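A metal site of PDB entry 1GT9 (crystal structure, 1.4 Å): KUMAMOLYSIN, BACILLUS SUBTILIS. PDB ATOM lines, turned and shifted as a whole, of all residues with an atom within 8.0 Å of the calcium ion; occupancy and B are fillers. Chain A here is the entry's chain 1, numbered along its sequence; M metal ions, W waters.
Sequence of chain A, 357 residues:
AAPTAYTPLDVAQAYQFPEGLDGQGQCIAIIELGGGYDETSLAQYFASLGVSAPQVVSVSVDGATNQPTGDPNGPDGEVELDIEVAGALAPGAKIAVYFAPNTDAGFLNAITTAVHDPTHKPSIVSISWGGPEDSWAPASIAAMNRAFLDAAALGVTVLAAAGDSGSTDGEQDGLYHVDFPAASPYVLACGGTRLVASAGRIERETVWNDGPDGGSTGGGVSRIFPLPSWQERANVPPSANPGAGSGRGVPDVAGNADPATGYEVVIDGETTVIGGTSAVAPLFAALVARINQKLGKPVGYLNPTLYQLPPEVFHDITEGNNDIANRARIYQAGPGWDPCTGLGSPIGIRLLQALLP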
ATOM      1  N   VAL A 207      -8.074  -2.043  -4.115  1.00  0.00           N
ATOM      2  CA  VAL A 207      -7.645  -0.687  -3.754  1.00  0.00           C
ATOM      3  C   VAL A 207      -7.867   0.265  -4.925  1.00  0.00           C
ATOM      4  O   VAL A 207      -7.587  -0.077  -6.082  1.00  0.00           O
ATOM      5  CB  VAL A 207      -6.123  -0.659  -3.405  1.00  0.00           C
ATOM      6  CG1 VAL A 207      -5.671   0.755  -3.017  1.00  0.00           C
ATOM      7  CG2 VAL A 207      -5.803  -1.652  -2.281  1.00  0.00           C
ATOM      8  N   HIS A 315     -15.777  -6.484   4.762  1.00  0.00           N
ATOM      9  CA  HIS A 315     -15.353  -7.144   3.552  1.00  0.00           C
ATOM     10  C   HIS A 315     -13.860  -6.758   3.436  1.00  0.00           C
ATOM     11  O   HIS A 315     -13.506  -5.588   3.209  1.00  0.00           O
ATOM     12  CB  HIS A 315     -16.158  -6.615   2.351  1.00  0.00           C
ATOM     13  CG  HIS A 315     -15.824  -7.288   1.060  1.00  0.00           C
ATOM     14  ND1 HIS A 315     -15.192  -6.644   0.018  1.00  0.00           N
ATOM     15  CD2 HIS A 315     -16.038  -8.558   0.650  1.00  0.00           C
ATOM     16  CE1 HIS A 315     -15.030  -7.498  -0.985  1.00  0.00           C
ATOM     17  NE2 HIS A 315     -15.534  -8.659  -0.625  1.00  0.00           N
ATOM     18  N   ASP A 316     -12.990  -7.719   3.632  1.00  0.00           N
ATOM     19  CA  ASP A 316     -11.546  -7.495   3.589  1.00  0.00           C
ATOM     20  C   ASP A 316     -11.061  -7.216   2.153  1.00  0.00           C
ATOM     21  O   ASP A 316     -11.346  -8.000   1.235  1.00  0.00           O
ATOM     22  CB  ASP A 316     -10.865  -8.751   4.177  1.00  0.00           C
ATOM     23  CG  ASP A 316      -9.395  -8.570   4.425  1.00  0.00           C
ATOM     24  OD1 ASP A 316      -8.886  -7.485   4.182  1.00  0.00           O
ATOM     25  OD2 ASP A 316      -8.727  -9.527   4.870  1.00  0.00           O
ATOM     26  N   ILE A 317     -10.399  -6.085   1.928  1.00  0.00           N
ATOM     27  CA  ILE A 317      -9.827  -5.835   0.596  1.00  0.00           C
ATOM     28  C   ILE A 317      -8.403  -6.361   0.714  1.00  0.00           C
ATOM     29  O   ILE A 317      -7.682  -6.047   1.640  1.00  0.00           O
ATOM     30  CB  ILE A 317      -9.805  -4.332   0.215  1.00  0.00           C
ATOM     31  CG1 ILE A 317     -11.209  -3.846  -0.153  1.00  0.00           C
ATOM     32  CG2 ILE A 317      -8.986  -4.148  -1.066  1.00  0.00           C
ATOM     33  CD1 ILE A 317     -12.110  -3.687   0.953  1.00  0.00           C
ATOM     34  N   THR A 318      -7.968  -7.170  -0.240  1.00  0.00           N
ATOM     35  CA  THR A 318      -6.649  -7.776  -0.157  1.00  0.00           C
ATOM     36  C   THR A 318      -5.767  -7.546  -1.362  1.00  0.00           C
ATOM     37  O   THR A 318      -4.572  -7.863  -1.324  1.00  0.00           O
ATOM     38  CB  THR A 318      -6.770  -9.317  -0.013  1.00  0.00           C
ATOM     39  OG1 THR A 318      -7.452  -9.855  -1.151  1.00  0.00           O
ATOM     40  CG2 THR A 318      -7.569  -9.672   1.243  1.00  0.00           C
ATOM     41  N   GLU A 319      -6.341  -6.977  -2.419  1.00  0.00           N
ATOM     42  CA  GLU A 319      -5.601  -6.767  -3.656  1.00  0.00           C
ATOM     43  C   GLU A 319      -5.441  -5.307  -4.040  1.00  0.00           C
ATOM     44  O   GLU A 319      -6.413  -4.539  -4.011  1.00  0.00           O
ATOM     45  CB  GLU A 319      -6.314  -7.527  -4.792  1.00  0.00           C
ATOM     46  CG  GLU A 319      -5.746  -7.377  -6.185  1.00  0.00           C
ATOM     47  CD  GLU A 319      -6.419  -8.321  -7.193  1.00  0.00           C
ATOM     48  OE1 GLU A 319      -7.540  -8.841  -6.903  1.00  0.00           O
ATOM     49  OE2 GLU A 319      -5.823  -8.545  -8.282  1.00  0.00           O
ATOM     50  N   GLN A 332       0.778  -1.656   0.411  1.00  0.00           N
ATOM     51  CA  GLN A 332       0.016  -2.707  -0.224  1.00  0.00           C
ATOM     52  C   GLN A 332      -1.119  -3.251   0.630  1.00  0.00           C
ATOM     53  O   GLN A 332      -1.002  -3.336   1.853  1.00  0.00           O
ATOM     54  CB  GLN A 332       0.991  -3.837  -0.562  1.00  0.00           C
ATOM     55  CG  GLN A 332       0.525  -4.838  -1.590  1.00  0.00           C
ATOM     56  CD  GLN A 332       1.649  -5.784  -1.969  1.00  0.00           C
ATOM     57  OE1 GLN A 332       1.945  -6.740  -1.235  1.00  0.00           O
ATOM     58  NE2 GLN A 332       2.302  -5.509  -3.091  1.00  0.00           N
ATOM     59  N   ALA A 333      -2.215  -3.609  -0.007  1.00  0.00           N
ATOM     60  CA  ALA A 333      -3.325  -4.245   0.691  1.00  0.00           C
ATOM     61  C   ALA A 333      -2.953  -5.703   0.985  1.00  0.00           C
ATOM     62  O   ALA A 333      -2.058  -6.291   0.358  1.00  0.00           O
ATOM     63  CB  ALA A 333      -4.620  -4.219  -0.162  1.00  0.00           C
ATOM     64  N   GLY A 334      -3.651  -6.291   1.932  1.00  0.00           N
ATOM     65  CA  GLY A 334      -3.375  -7.677   2.246  1.00  0.00           C
ATOM     66  C   GLY A 334      -4.430  -8.187   3.194  1.00  0.00           C
ATOM     67  O   GLY A 334      -5.397  -7.506   3.470  1.00  0.00           O
ATOM     68  N   PRO A 335      -4.257  -9.408   3.707  1.00  0.00           N
ATOM     69  CA  PRO A 335      -5.243  -9.954   4.638  1.00  0.00           C
ATOM     70  C   PRO A 335      -5.308  -9.116   5.906  1.00  0.00           C
ATOM     71  O   PRO A 335      -4.259  -8.717   6.422  1.00  0.00           O
ATOM     72  CB  PRO A 335      -4.718 -11.376   4.887  1.00  0.00           C
ATOM     73  CG  PRO A 335      -3.228 -11.251   4.657  1.00  0.00           C
ATOM     74  CD  PRO A 335      -3.142 -10.330   3.461  1.00  0.00           C
ATOM     75  N   GLY A 336      -6.510  -8.868   6.388  1.00  0.00           N
ATOM     76  CA  GLY A 336      -6.677  -8.079   7.593  1.00  0.00           C
ATOM     77  C   GLY A 336      -6.497  -6.591   7.330  1.00  0.00           C
ATOM     78  O   GLY A 336      -6.605  -6.124   6.192  1.00  0.00           O
ATOM     79  N   TRP A 337      -6.194  -5.837   8.364  1.00  0.00           N
ATOM     80  CA  TRP A 337      -6.008  -4.402   8.218  1.00  0.00           C
ATOM     81  C   TRP A 337      -4.805  -4.109   7.345  1.00  0.00           C
ATOM     82  O   TRP A 337      -3.789  -4.779   7.422  1.00  0.00           O
ATOM     83  CB  TRP A 337      -5.785  -3.783   9.616  1.00  0.00           C
ATOM     84  CG  TRP A 337      -5.745  -2.272   9.602  1.00  0.00           C
ATOM     85  CD1 TRP A 337      -6.793  -1.407   9.875  1.00  0.00           C
ATOM     86  CD2 TRP A 337      -4.628  -1.448   9.222  1.00  0.00           C
ATOM     87  NE1 TRP A 337      -6.393  -0.105   9.669  1.00  0.00           N
ATOM     88  CE2 TRP A 337      -5.079  -0.103   9.270  1.00  0.00           C
ATOM     89  CE3 TRP A 337      -3.298  -1.724   8.854  1.00  0.00           C
ATOM     90  CZ2 TRP A 337      -4.249   0.974   8.935  1.00  0.00           C
ATOM     91  CZ3 TRP A 337      -2.479  -0.651   8.532  1.00  0.00           C
ATOM     92  CH2 TRP A 337      -2.950   0.677   8.567  1.00  0.00           C
ATOM     93  N   ASP A 338      -4.936  -3.100   6.491  1.00  0.00           N
ATOM     94  CA  ASP A 338      -3.797  -2.664   5.692  1.00  0.00           C
ATOM     95  C   ASP A 338      -3.826  -1.141   5.516  1.00  0.00           C
ATOM     96  O   ASP A 338      -4.866  -0.510   5.774  1.00  0.00           O
ATOM     97  CB  ASP A 338      -3.715  -3.387   4.341  1.00  0.00           C
ATOM     98  CG  ASP A 338      -4.974  -3.242   3.527  1.00  0.00           C
ATOM     99  OD1 ASP A 338      -5.302  -2.106   3.072  1.00  0.00           O
ATOM    100  OD2 ASP A 338      -5.637  -4.257   3.321  1.00  0.00           O
ATOM    101  N   PRO A 339      -2.690  -0.534   5.135  1.00  0.00           N
ATOM    102  CA  PRO A 339      -2.643   0.917   4.961  1.00  0.00           C
ATOM    103  C   PRO A 339      -3.195   1.481   3.658  1.00  0.00           C
ATOM    104  O   PRO A 339      -2.785   2.560   3.217  1.00  0.00           O
ATOM    105  CB  PRO A 339      -1.164   1.263   5.180  1.00  0.00           C
ATOM    106  CG  PRO A 339      -0.465  -0.078   5.474  1.00  0.00           C
ATOM    107  CD  PRO A 339      -1.356  -1.109   4.886  1.00  0.00           C
ATOM    108  N   CYS A 340      -4.101   0.733   3.026  1.00  0.00           N
ATOM    109  CA  CYS A 340      -4.778   1.233   1.826  1.00  0.00           C
ATOM    110  C   CYS A 340      -6.269   1.292   2.129  1.00  0.00           C
ATOM    111  O   CYS A 340      -6.958   2.242   1.756  1.00  0.00           O
ATOM    112  CB  CYS A 340      -4.579   0.294   0.641  1.00  0.00           C
ATOM    113  SG  CYS A 340      -2.889  -0.002   0.140  1.00  0.00           S
ATOM    114  N   THR A 341      -6.757   0.279   2.841  1.00  0.00           N
ATOM    115  CA  THR A 341      -8.188   0.150   3.049  1.00  0.00           C
ATOM    116  C   THR A 341      -8.602  -0.119   4.490  1.00  0.00           C
ATOM    117  O   THR A 341      -9.786  -0.314   4.771  1.00  0.00           O
ATOM    118  CB  THR A 341      -8.781  -0.976   2.133  1.00  0.00           C
ATOM    119  OG1 THR A 341      -8.118  -2.225   2.448  1.00  0.00           O
ATOM    120  CG2 THR A 341      -8.573  -0.629   0.646  1.00  0.00           C
ATOM    121  N   GLY A 342      -7.638  -0.141   5.404  1.00  0.00           N
ATOM    122  CA  GLY A 342      -7.961  -0.385   6.818  1.00  0.00           C
ATOM    123  C   GLY A 342      -8.624  -1.740   7.001  1.00  0.00           C
ATOM    124  O   GLY A 342      -8.172  -2.747   6.431  1.00  0.00           O
ATOM    125  N   LEU A 343      -9.721  -1.745   7.746  1.00  0.00           N
ATOM    126  CA  LEU A 343     -10.488  -2.978   8.025  1.00  0.00           C
ATOM    127  C   LEU A 343     -11.286  -3.453   6.801  1.00  0.00           C
ATOM    128  O   LEU A 343     -11.794  -4.554   6.816  1.00  0.00           O
ATOM    129  CB  LEU A 343     -11.435  -2.744   9.206  1.00  0.00           C
ATOM    130  CG  LEU A 343     -10.715  -2.394  10.530  1.00  0.00           C
ATOM    131  CD1 LEU A 343     -11.700  -1.944  11.601  1.00  0.00           C
ATOM    132  CD2 LEU A 343      -9.911  -3.613  11.006  1.00  0.00           C
ATOM    133  N   GLY A 344     -11.346  -2.629   5.748  1.00  0.00           N
ATOM    134  CA  GLY A 344     -12.085  -2.950   4.544  1.00  0.00           C
ATOM    135  C   GLY A 344     -13.418  -2.205   4.469  1.00  0.00           C
ATOM    136  O   GLY A 344     -13.598  -1.171   5.121  1.00  0.00           O
ATOM    137  N   SER A 345     -14.350  -2.717   3.660  1.00  0.00           N
ATOM    138  CA  SER A 345     -15.647  -2.067   3.554  1.00  0.00           C
ATOM    139  C   SER A 345     -16.628  -2.694   4.549  1.00  0.00           C
ATOM    140  O   SER A 345     -16.684  -3.925   4.712  1.00  0.00           O
ATOM    141  CB  SER A 345     -16.222  -2.131   2.125  1.00  0.00           C
ATOM    142  OG  SER A 345     -16.308  -3.467   1.600  1.00  0.00           O
HETATM  143 CA    CA M   1      -7.142  -5.962   3.937  1.00  0.00          CA
HETATM  144  O   HOH W   1      -8.784  -4.202   4.222  1.00  0.00           O
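The calcium ion is bound by O of Gly 336 (2.3 Å), OD1 of Asp 316 (2.3 Å), OD2 of Asp 338 (2.4 Å), O of Ile 317 (2.4 Å), O of Gly 334 (2.4 Å) and water W1 (2.4 Å).
The calcium ion has six donor atoms within binding distance.
The nearest printed residue that does not touch the calcium ion is Thr 341 (4.1 Å).
Water W1 lies within hydrogen-bond range of O of Gly 342 (2.7 Å), OG1 of Thr 341 (2.7 Å), N of Gly 344 (3.4 Å) and N of Ile 317 (3.4 Å).
The side-chain carboxylate (OD1) of Asp 338 sits at hydrogen-bond distance from the backbone NH (N) of Cys 340, at 3.1 Å.
OD1 of Asp 338 lies within hydrogen-bond range of N of Thr 341, at 2.8 Å.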
